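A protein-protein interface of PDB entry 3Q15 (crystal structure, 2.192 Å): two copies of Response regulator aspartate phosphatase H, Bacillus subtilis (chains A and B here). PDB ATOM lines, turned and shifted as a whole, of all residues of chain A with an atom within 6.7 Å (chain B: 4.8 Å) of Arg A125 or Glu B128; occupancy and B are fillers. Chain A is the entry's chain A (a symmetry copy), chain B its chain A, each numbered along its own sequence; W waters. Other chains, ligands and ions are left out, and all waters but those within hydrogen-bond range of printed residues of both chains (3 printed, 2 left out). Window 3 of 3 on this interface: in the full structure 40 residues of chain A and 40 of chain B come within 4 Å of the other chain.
Of the printed residues of chain B, Ile A121 touches Tyr B162 (3.8 Å). Arg A125 touches just these residues of chain B: Arg B125 (2.8 Å), Glu B128 (2.9 Å), Tyr B162 (3.8 Å) and His B163 (3.9 Å). Printed residues of chain B within 4 Å of Glu A128: Arg B125 (2.9 Å). Lys A129 touches none of the printed residues of chain B. Printed residues of chain B within 4 Å of His A163: Arg B125 (3.9 Å). Of chain A, only Arg A125 comes within 4 Å of Glu B128. Of the printed residues of chain A, Tyr B162 touches Ile A121, Gly A122 and Arg A125. The nearest printed residue of chain B that does not touch Arg A125 is Lys B129 (5.4 Å). The nearest residue of chain A that does not touch Glu B128 is Lys A129 (4.4 Å). The nearest printed residue of chain B that does not touch His A163 is Lys B129 (8.3 Å).
Hydrophobic or aromatic side chains of chain A within 4 Å of the printed part of chain B: Ile A121 and His A163. Printed residues of chain B that touch a printed residue of chain A: Arg B125, Glu B128, Tyr B162 and His B163. Hydrophobic or aromatic side chains of chain B within 4 Å of the printed part of chain A: Tyr B162 and His B163. Among the printed residues, 8 pairs touch across the chains. Among the printed residues, Asp or Glu carboxylates within 4 Å of a Lys or Arg side-chain nitrogen of the other chain: Arg A125 with Glu B128 (2.9 Å) and Glu A128 with Arg B125 (2.9 Å).
Arg B125 touches its own counterpart, Arg A125. Arg A125 touches Glu B128, and with the chains exchanged Glu A128 touches Arg B125. Arg A125 touches His B163, and with the chains exchanged His A163 touches Arg B125. Of the 8 pairs that touch across the chains among the printed residues, 5 have their exchanged pair printed and touching as well.
Water W2 lies within hydrogen-bond range of the guanidinium group of Arg B125 (2.5 Å) and a ring nitrogen (NE2) of His A163 (3.0 Å). Water W3 lies within hydrogen-bond range of NH1 of Arg A125 and NE2 of His B163. Water W1 lies within hydrogen-bond range of OE1 of Glu A126, O of Gly A122 and OH of Tyr B162.
The side-chain carboxylate (OE1) of Glu A128 lies within salt-bridge range of the guanidinium group (NH2) of Arg B125 (2.9 Å). NH2 of Arg A125 lies close to NE of Arg B125. OE1 of Glu B128 is in salt-bridge range of NH2 of Arg A125.
A ring nitrogen (ND1) of His B163 is in hydrogen-bond range of a ring nitrogen (ND1) of His B144, 2.9 Å away.
Among the printed residues, merely in contact across the chains: Gly A122 with Tyr B162 (3.2 Å), Ile A121 with Tyr B162 (3.8 Å), Arg A125 with Tyr B162 (3.8 Å), Arg A125 with His B163 (3.9 Å) and His A163 with Arg B125 (3.9 Å).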
ATOM      1  N   ALA A 120       2.603 -12.595  -8.800  1.00  0.00           N
ATOM      2  CA  ALA A 120       3.953 -12.200  -8.394  1.00  0.00           C
ATOM      3  C   ALA A 120       4.763 -11.651  -9.563  1.00  0.00           C
ATOM      4  O   ALA A 120       5.365 -10.584  -9.463  1.00  0.00           O
ATOM      5  CB  ALA A 120       4.689 -13.369  -7.741  1.00  0.00           C
ATOM      6  N   ILE A 121       4.778 -12.391 -10.665  1.00  0.00           N
ATOM      7  CA  ILE A 121       5.503 -11.981 -11.865  1.00  0.00           C
ATOM      8  C   ILE A 121       5.085 -10.576 -12.300  1.00  0.00           C
ATOM      9  O   ILE A 121       5.927  -9.719 -12.580  1.00  0.00           O
ATOM     10  CB  ILE A 121       5.275 -12.991 -13.015  1.00  0.00           C
ATOM     11  CG1 ILE A 121       5.899 -14.345 -12.656  1.00  0.00           C
ATOM     12  CG2 ILE A 121       5.843 -12.475 -14.331  1.00  0.00           C
ATOM     13  CD1 ILE A 121       5.461 -15.497 -13.555  1.00  0.00           C
ATOM     14  N   GLY A 122       3.776 -10.349 -12.338  1.00  0.00           N
ATOM     15  CA  GLY A 122       3.235  -9.057 -12.707  1.00  0.00           C
ATOM     16  C   GLY A 122       3.782  -7.934 -11.850  1.00  0.00           C
ATOM     17  O   GLY A 122       4.105  -6.863 -12.359  1.00  0.00           O
ATOM     18  N   TYR A 123       3.889  -8.174 -10.548  1.00  0.00           N
ATOM     19  CA  TYR A 123       4.442  -7.164  -9.649  1.00  0.00           C
ATOM     20  C   TYR A 123       5.955  -7.038  -9.816  1.00  0.00           C
ATOM     21  O   TYR A 123       6.499  -5.933  -9.768  1.00  0.00           O
ATOM     22  CB  TYR A 123       4.046  -7.429  -8.191  1.00  0.00           C
ATOM     23  CG  TYR A 123       2.606  -7.048  -7.904  1.00  0.00           C
ATOM     24  CD1 TYR A 123       2.244  -5.718  -7.714  1.00  0.00           C
ATOM     25  CD2 TYR A 123       1.608  -8.012  -7.843  1.00  0.00           C
ATOM     26  CE1 TYR A 123       0.930  -5.362  -7.467  1.00  0.00           C
ATOM     27  CE2 TYR A 123       0.295  -7.668  -7.594  1.00  0.00           C
ATOM     28  CZ  TYR A 123      -0.041  -6.345  -7.409  1.00  0.00           C
ATOM     29  OH  TYR A 123      -1.349  -6.009  -7.162  1.00  0.00           O
ATOM     30  N   TYR A 124       6.628  -8.166 -10.031  1.00  0.00           N
ATOM     31  CA  TYR A 124       8.063  -8.147 -10.297  1.00  0.00           C
ATOM     32  C   TYR A 124       8.374  -7.267 -11.502  1.00  0.00           C
ATOM     33  O   TYR A 124       9.319  -6.482 -11.479  1.00  0.00           O
ATOM     34  CB  TYR A 124       8.606  -9.556 -10.544  1.00  0.00           C
ATOM     35  CG  TYR A 124       8.651 -10.441  -9.321  1.00  0.00           C
ATOM     36  CD1 TYR A 124       8.680  -9.900  -8.044  1.00  0.00           C
ATOM     37  CD2 TYR A 124       8.663 -11.826  -9.447  1.00  0.00           C
ATOM     38  CE1 TYR A 124       8.719 -10.716  -6.924  1.00  0.00           C
ATOM     39  CE2 TYR A 124       8.702 -12.646  -8.336  1.00  0.00           C
ATOM     40  CZ  TYR A 124       8.729 -12.088  -7.078  1.00  0.00           C
ATOM     41  OH  TYR A 124       8.769 -12.915  -5.978  1.00  0.00           O
ATOM     42  N   ARG A 125       7.578  -7.412 -12.559  1.00  0.00           N
ATOM     43  CA  ARG A 125       7.789  -6.638 -13.777  1.00  0.00           C
ATOM     44  C   ARG A 125       7.566  -5.146 -13.524  1.00  0.00           C
ATOM     45  O   ARG A 125       8.390  -4.318 -13.903  1.00  0.00           O
ATOM     46  CB  ARG A 125       6.879  -7.137 -14.900  1.00  0.00           C
ATOM     47  CG  ARG A 125       7.120  -8.587 -15.293  1.00  0.00           C
ATOM     48  CD  ARG A 125       8.533  -8.786 -15.833  1.00  0.00           C
ATOM     49  NE  ARG A 125       8.885  -7.727 -16.771  1.00  0.00           N
ATOM     50  CZ  ARG A 125       8.549  -7.724 -18.057  1.00  0.00           C
ATOM     51  NH1 ARG A 125       7.858  -8.734 -18.564  1.00  0.00           N
ATOM     52  NH2 ARG A 125       8.907  -6.713 -18.836  1.00  0.00           N
ATOM     53  N   GLU A 126       6.458  -4.808 -12.873  1.00  0.00           N
ATOM     54  CA  GLU A 126       6.168  -3.414 -12.553  1.00  0.00           C
ATOM     55  C   GLU A 126       7.253  -2.827 -11.659  1.00  0.00           C
ATOM     56  O   GLU A 126       7.624  -1.662 -11.802  1.00  0.00           O
ATOM     57  CB  GLU A 126       4.794  -3.270 -11.885  1.00  0.00           C
ATOM     58  CG  GLU A 126       3.619  -3.651 -12.778  1.00  0.00           C
ATOM     59  CD  GLU A 126       3.606  -2.883 -14.092  1.00  0.00           C
ATOM     60  OE1 GLU A 126       3.679  -3.525 -15.163  1.00  0.00           O
ATOM     61  OE2 GLU A 126       3.515  -1.637 -14.060  1.00  0.00           O
ATOM     62  N   ALA A 127       7.759  -3.640 -10.736  1.00  0.00           N
ATOM     63  CA  ALA A 127       8.808  -3.200  -9.824  1.00  0.00           C
ATOM     64  C   ALA A 127      10.091  -2.861 -10.581  1.00  0.00           C
ATOM     65  O   ALA A 127      10.718  -1.827 -10.332  1.00  0.00           O
ATOM     66  CB  ALA A 127       9.070  -4.260  -8.762  1.00  0.00           C
ATOM     67  N   GLU A 128      10.474  -3.730 -11.512  1.00  0.00           N
ATOM     68  CA  GLU A 128      11.685  -3.514 -12.299  1.00  0.00           C
ATOM     69  C   GLU A 128      11.652  -2.177 -13.048  1.00  0.00           C
ATOM     70  O   GLU A 128      12.676  -1.502 -13.162  1.00  0.00           O
ATOM     71  CB  GLU A 128      11.936  -4.675 -13.271  1.00  0.00           C
ATOM     72  CG  GLU A 128      13.316  -4.626 -13.941  1.00  0.00           C
ATOM     73  CD  GLU A 128      13.591  -5.816 -14.849  1.00  0.00           C
ATOM     74  OE1 GLU A 128      12.839  -6.813 -14.776  1.00  0.00           O
ATOM     75  OE2 GLU A 128      14.561  -5.755 -15.637  1.00  0.00           O
ATOM     76  N   LYS A 129      10.476  -1.785 -13.537  1.00  0.00           N
ATOM     77  CA  LYS A 129      10.346  -0.535 -14.295  1.00  0.00           C
ATOM     78  C   LYS A 129      10.722   0.685 -13.461  1.00  0.00           C
ATOM     79  O   LYS A 129      10.989   1.757 -14.003  1.00  0.00           O
ATOM     80  CB  LYS A 129       8.926  -0.358 -14.845  1.00  0.00           C
ATOM     81  CG  LYS A 129       8.449  -1.480 -15.754  1.00  0.00           C
ATOM     82  CD  LYS A 129       7.086  -1.155 -16.357  1.00  0.00           C
ATOM     83  CE  LYS A 129       6.355  -2.416 -16.805  1.00  0.00           C
ATOM     84  NZ  LYS A 129       7.171  -3.252 -17.727  1.00  0.00           N
ATOM     85  N   GLU A 130      10.730   0.522 -12.141  1.00  0.00           N
ATOM     86  CA  GLU A 130      11.091   1.606 -11.231  1.00  0.00           C
ATOM     87  C   GLU A 130      12.601   1.709 -11.028  1.00  0.00           C
ATOM     88  O   GLU A 130      13.110   2.748 -10.605  1.00  0.00           O
ATOM     89  CB  GLU A 130      10.399   1.432  -9.879  1.00  0.00           C
ATOM     90  CG  GLU A 130       8.886   1.524  -9.941  1.00  0.00           C
ATOM     91  CD  GLU A 130       8.417   2.831 -10.548  1.00  0.00           C
ATOM     92  OE1 GLU A 130       7.407   2.815 -11.283  1.00  0.00           O
ATOM     93  OE2 GLU A 130       9.059   3.871 -10.289  1.00  0.00           O
ATOM     94  N   PHE A 143      17.763  -6.531  -6.580  1.00  0.00           N
ATOM     95  CA  PHE A 143      16.478  -6.895  -7.152  1.00  0.00           C
ATOM     96  C   PHE A 143      16.589  -8.139  -8.030  1.00  0.00           C
ATOM     97  O   PHE A 143      15.775  -9.061  -7.933  1.00  0.00           O
ATOM     98  CB  PHE A 143      15.920  -5.742  -7.979  1.00  0.00           C
ATOM     99  CG  PHE A 143      14.760  -6.135  -8.840  1.00  0.00           C
ATOM    100  CD1 PHE A 143      13.479  -6.195  -8.313  1.00  0.00           C
ATOM    101  CD2 PHE A 143      14.950  -6.464 -10.170  1.00  0.00           C
ATOM    102  CE1 PHE A 143      12.406  -6.564  -9.100  1.00  0.00           C
ATOM    103  CE2 PHE A 143      13.883  -6.836 -10.962  1.00  0.00           C
ATOM    104  CZ  PHE A 143      12.606  -6.882 -10.428  1.00  0.00           C
ATOM    105  N   TYR A 151      12.204 -16.908  -9.085  1.00  0.00           N
ATOM    106  CA  TYR A 151      11.973 -17.636 -10.329  1.00  0.00           C
ATOM    107  C   TYR A 151      12.506 -19.066 -10.248  1.00  0.00           C
ATOM    108  O   TYR A 151      11.921 -19.989 -10.817  1.00  0.00           O
ATOM    109  CB  TYR A 151      12.588 -16.901 -11.524  1.00  0.00           C
ATOM    110  CG  TYR A 151      11.727 -15.779 -12.061  1.00  0.00           C
ATOM    111  CD1 TYR A 151      10.519 -16.050 -12.685  1.00  0.00           C
ATOM    112  CD2 TYR A 151      12.125 -14.451 -11.954  1.00  0.00           C
ATOM    113  CE1 TYR A 151       9.724 -15.035 -13.181  1.00  0.00           C
ATOM    114  CE2 TYR A 151      11.334 -13.420 -12.448  1.00  0.00           C
ATOM    115  CZ  TYR A 151      10.138 -13.721 -13.061  1.00  0.00           C
ATOM    116  OH  TYR A 151       9.350 -12.711 -13.554  1.00  0.00           O
ATOM    117  N   HIS A 163      17.972 -13.404 -14.901  1.00  0.00           N
ATOM    118  CA  HIS A 163      18.102 -12.434 -13.819  1.00  0.00           C
ATOM    119  C   HIS A 163      19.379 -12.589 -13.002  1.00  0.00           C
ATOM    120  O   HIS A 163      20.031 -11.600 -12.680  1.00  0.00           O
ATOM    121  CB  HIS A 163      16.878 -12.474 -12.905  1.00  0.00           C
ATOM    122  CG  HIS A 163      15.691 -11.769 -13.477  1.00  0.00           C
ATOM    123  ND1 HIS A 163      15.587 -10.395 -13.513  1.00  0.00           N
ATOM    124  CD2 HIS A 163      14.561 -12.246 -14.054  1.00  0.00           C
ATOM    125  CE1 HIS A 163      14.444 -10.055 -14.082  1.00  0.00           C
ATOM    126  NE2 HIS A 163      13.803 -11.162 -14.418  1.00  0.00           N
ATOM    127  N   TYR B 124      13.565 -10.260 -25.534  1.00  0.00           N
ATOM    128  CA  TYR B 124      12.135 -10.096 -25.291  1.00  0.00           C
ATOM    129  C   TYR B 124      11.883  -8.936 -24.334  1.00  0.00           C
ATOM    130  O   TYR B 124      10.983  -8.128 -24.552  1.00  0.00           O
ATOM    131  CB  TYR B 124      11.514 -11.372 -24.715  1.00  0.00           C
ATOM    132  CG  TYR B 124      11.411 -12.521 -25.689  1.00  0.00           C
ATOM    133  CD1 TYR B 124      11.404 -12.302 -27.060  1.00  0.00           C
ATOM    134  CD2 TYR B 124      11.321 -13.831 -25.235  1.00  0.00           C
ATOM    135  CE1 TYR B 124      11.311 -13.360 -27.950  1.00  0.00           C
ATOM    136  CE2 TYR B 124      11.228 -14.892 -26.116  1.00  0.00           C
ATOM    137  CZ  TYR B 124      11.224 -14.652 -27.471  1.00  0.00           C
ATOM    138  OH  TYR B 124      11.130 -15.715 -28.340  1.00  0.00           O
ATOM    139  N   ARG B 125      12.677  -8.867 -23.268  1.00  0.00           N
ATOM    140  CA  ARG B 125      12.518  -7.813 -22.274  1.00  0.00           C
ATOM    141  C   ARG B 125      12.823  -6.440 -22.877  1.00  0.00           C
ATOM    142  O   ARG B 125      12.051  -5.500 -22.714  1.00  0.00           O
ATOM    143  CB  ARG B 125      13.406  -8.078 -21.058  1.00  0.00           C
ATOM    144  CG  ARG B 125      13.086  -9.374 -20.328  1.00  0.00           C
ATOM    145  CD  ARG B 125      11.668  -9.357 -19.766  1.00  0.00           C
ATOM    146  NE  ARG B 125      11.383  -8.085 -19.113  1.00  0.00           N
ATOM    147  CZ  ARG B 125      11.727  -7.792 -17.864  1.00  0.00           C
ATOM    148  NH1 ARG B 125      12.364  -8.688 -17.124  1.00  0.00           N
ATOM    149  NH2 ARG B 125      11.433  -6.605 -17.353  1.00  0.00           N
ATOM    150  N   GLU B 126      13.944  -6.333 -23.582  1.00  0.00           N
ATOM    151  CA  GLU B 126      14.311  -5.075 -24.226  1.00  0.00           C
ATOM    152  C   GLU B 126      13.255  -4.660 -25.243  1.00  0.00           C
ATOM    153  O   GLU B 126      12.952  -3.476 -25.387  1.00  0.00           O
ATOM    154  CB  GLU B 126      15.686  -5.174 -24.900  1.00  0.00           C
ATOM    155  CG  GLU B 126      16.844  -5.395 -23.933  1.00  0.00           C
ATOM    156  CD  GLU B 126      16.910  -4.335 -22.842  1.00  0.00           C
ATOM    157  OE1 GLU B 126      16.808  -4.697 -21.649  1.00  0.00           O
ATOM    158  OE2 GLU B 126      17.071  -3.142 -23.173  1.00  0.00           O
ATOM    159  N   ALA B 127      12.697  -5.641 -25.946  1.00  0.00           N
ATOM    160  CA  ALA B 127      11.668  -5.375 -26.944  1.00  0.00           C
ATOM    161  C   ALA B 127      10.412  -4.791 -26.300  1.00  0.00           C
ATOM    162  O   ALA B 127       9.844  -3.813 -26.795  1.00  0.00           O
ATOM    163  CB  ALA B 127      11.340  -6.642 -27.722  1.00  0.00           C
ATOM    164  N   GLU B 128       9.987  -5.387 -25.191  1.00  0.00           N
ATOM    165  CA  GLU B 128       8.795  -4.920 -24.487  1.00  0.00           C
ATOM    166  C   GLU B 128       8.910  -3.446 -24.081  1.00  0.00           C
ATOM    167  O   GLU B 128       7.927  -2.707 -24.140  1.00  0.00           O
ATOM    168  CB  GLU B 128       8.486  -5.797 -23.266  1.00  0.00           C
ATOM    169  CG  GLU B 128       7.116  -5.509 -22.637  1.00  0.00           C
ATOM    170  CD  GLU B 128       6.780  -6.429 -21.472  1.00  0.00           C
ATOM    171  OE1 GLU B 128       7.474  -7.455 -21.297  1.00  0.00           O
ATOM    172  OE2 GLU B 128       5.820  -6.125 -20.728  1.00  0.00           O
ATOM    173  N   LYS B 129      10.110  -3.016 -23.693  1.00  0.00           N
ATOM    174  CA  LYS B 129      10.316  -1.629 -23.257  1.00  0.00           C
ATOM    175  C   LYS B 129      10.004  -0.626 -24.363  1.00  0.00           C
ATOM    176  O   LYS B 129       9.801   0.558 -24.096  1.00  0.00           O
ATOM    177  CB  LYS B 129      11.746  -1.406 -22.756  1.00  0.00           C
ATOM    178  CG  LYS B 129      12.166  -2.301 -21.600  1.00  0.00           C
ATOM    179  CD  LYS B 129      13.549  -1.919 -21.083  1.00  0.00           C
ATOM    180  CE  LYS B 129      14.210  -3.075 -20.340  1.00  0.00           C
ATOM    181  NZ  LYS B 129      13.354  -3.616 -19.250  1.00  0.00           N
ATOM    182  N   GLU B 130       9.977  -1.102 -25.604  1.00  0.00           N
ATOM    183  CA  GLU B 130       9.672  -0.249 -26.751  1.00  0.00           C
ATOM    184  C   GLU B 130       8.169  -0.112 -26.984  1.00  0.00           C
ATOM    185  O   GLU B 130       7.717   0.821 -27.648  1.00  0.00           O
ATOM    186  CB  GLU B 130      10.344  -0.783 -28.017  1.00  0.00           C
ATOM    187  CG  GLU B 130      11.860  -0.764 -27.968  1.00  0.00           C
ATOM    188  CD  GLU B 130      12.406   0.621 -27.690  1.00  0.00           C
ATOM    189  OE1 GLU B 130      13.419   0.725 -26.966  1.00  0.00           O
ATOM    190  OE2 GLU B 130      11.822   1.603 -28.196  1.00  0.00           O
ATOM    191  N   LEU B 131       7.399  -1.046 -26.438  1.00  0.00           N
ATOM    192  CA  LEU B 131       5.950  -1.035 -26.611  1.00  0.00           C
ATOM    193  C   LEU B 131       5.277   0.250 -26.123  1.00  0.00           C
ATOM    194  O   LEU B 131       4.418   0.790 -26.812  1.00  0.00           O
ATOM    195  CB  LEU B 131       5.307  -2.255 -25.945  1.00  0.00           C
ATOM    196  CG  LEU B 131       5.323  -3.565 -26.734  1.00  0.00           C
ATOM    197  CD1 LEU B 131       4.618  -3.402 -28.070  1.00  0.00           C
ATOM    198  CD2 LEU B 131       6.742  -4.032 -26.942  1.00  0.00           C
ATOM    199  N   PRO B 132       5.655   0.735 -24.926  1.00  0.00           N
ATOM    200  CA  PRO B 132       5.023   1.933 -24.358  1.00  0.00           C
ATOM    201  C   PRO B 132       5.056   3.124 -25.306  1.00  0.00           C
ATOM    202  O   PRO B 132       4.268   4.059 -25.154  1.00  0.00           O
ATOM    203  CB  PRO B 132       5.884   2.229 -23.127  1.00  0.00           C
ATOM    204  CG  PRO B 132       6.413   0.898 -22.722  1.00  0.00           C
ATOM    205  CD  PRO B 132       6.652   0.158 -24.006  1.00  0.00           C
ATOM    206  N   PHE B 143       2.517  -8.874 -29.354  1.00  0.00           N
ATOM    207  CA  PHE B 143       3.783  -9.162 -28.702  1.00  0.00           C
ATOM    208  C   PHE B 143       3.607 -10.150 -27.552  1.00  0.00           C
ATOM    209  O   PHE B 143       4.367 -11.113 -27.418  1.00  0.00           O
ATOM    210  CB  PHE B 143       4.411  -7.878 -28.173  1.00  0.00           C
ATOM    211  CG  PHE B 143       5.553  -8.117 -27.235  1.00  0.00           C
ATOM    212  CD1 PHE B 143       6.825  -8.375 -27.723  1.00  0.00           C
ATOM    213  CD2 PHE B 143       5.354  -8.106 -25.866  1.00  0.00           C
ATOM    214  CE1 PHE B 143       7.881  -8.604 -26.863  1.00  0.00           C
ATOM    215  CE2 PHE B 143       6.404  -8.335 -25.000  1.00  0.00           C
ATOM    216  CZ  PHE B 143       7.672  -8.581 -25.499  1.00  0.00           C
ATOM    217  N   HIS B 144       2.608  -9.899 -26.713  1.00  0.00           N
ATOM    218  CA  HIS B 144       2.355 -10.756 -25.561  1.00  0.00           C
ATOM    219  C   HIS B 144       1.959 -12.170 -25.975  1.00  0.00           C
ATOM    220  O   HIS B 144       2.358 -13.147 -25.344  1.00  0.00           O
ATOM    221  CB  HIS B 144       1.294 -10.142 -24.646  1.00  0.00           C
ATOM    222  CG  HIS B 144       1.784  -8.959 -23.876  1.00  0.00           C
ATOM    223  ND1 HIS B 144       2.745  -9.060 -22.891  1.00  0.00           N
ATOM    224  CD2 HIS B 144       1.455  -7.649 -23.948  1.00  0.00           C
ATOM    225  CE1 HIS B 144       2.985  -7.862 -22.392  1.00  0.00           C
ATOM    226  NE2 HIS B 144       2.216  -6.987 -23.013  1.00  0.00           N
ATOM    227  N   TYR B 162       1.344 -15.391 -17.551  1.00  0.00           N
ATOM    228  CA  TYR B 162       1.374 -13.953 -17.321  1.00  0.00           C
ATOM    229  C   TYR B 162       1.157 -13.207 -18.626  1.00  0.00           C
ATOM    230  O   TYR B 162       0.256 -12.378 -18.734  1.00  0.00           O
ATOM    231  CB  TYR B 162       2.704 -13.540 -16.697  1.00  0.00           C
ATOM    232  CG  TYR B 162       2.960 -12.051 -16.735  1.00  0.00           C
ATOM    233  CD1 TYR B 162       2.424 -11.207 -15.771  1.00  0.00           C
ATOM    234  CD2 TYR B 162       3.742 -11.491 -17.733  1.00  0.00           C
ATOM    235  CE1 TYR B 162       2.658  -9.843 -15.804  1.00  0.00           C
ATOM    236  CE2 TYR B 162       3.983 -10.134 -17.773  1.00  0.00           C
ATOM    237  CZ  TYR B 162       3.439  -9.315 -16.805  1.00  0.00           C
ATOM    238  OH  TYR B 162       3.675  -7.958 -16.840  1.00  0.00           O
ATOM    239  N   HIS B 163       1.975 -13.520 -19.626  1.00  0.00           N
ATOM    240  CA  HIS B 163       1.893 -12.834 -20.910  1.00  0.00           C
ATOM    241  C   HIS B 163       0.603 -13.107 -21.674  1.00  0.00           C
ATOM    242  O   HIS B 163       0.007 -12.190 -22.229  1.00  0.00           O
ATOM    243  CB  HIS B 163       3.107 -13.161 -21.779  1.00  0.00           C
ATOM    244  CG  HIS B 163       4.336 -12.408 -21.386  1.00  0.00           C
ATOM    245  ND1 HIS B 163       4.518 -11.073 -21.681  1.00  0.00           N
ATOM    246  CD2 HIS B 163       5.440 -12.796 -20.702  1.00  0.00           C
ATOM    247  CE1 HIS B 163       5.682 -10.672 -21.201  1.00  0.00           C
ATOM    248  NE2 HIS B 163       6.262 -11.701 -20.605  1.00  0.00           N
HETATM  249  O   HOH W   1       3.214  -6.032 -14.806  1.00  0.00           O
HETATM  250  O   HOH W   2      12.090 -11.117 -16.844  1.00  0.00           O
HETATM  251  O   HOH W   3       7.992 -11.171 -18.249  1.00  0.00           O
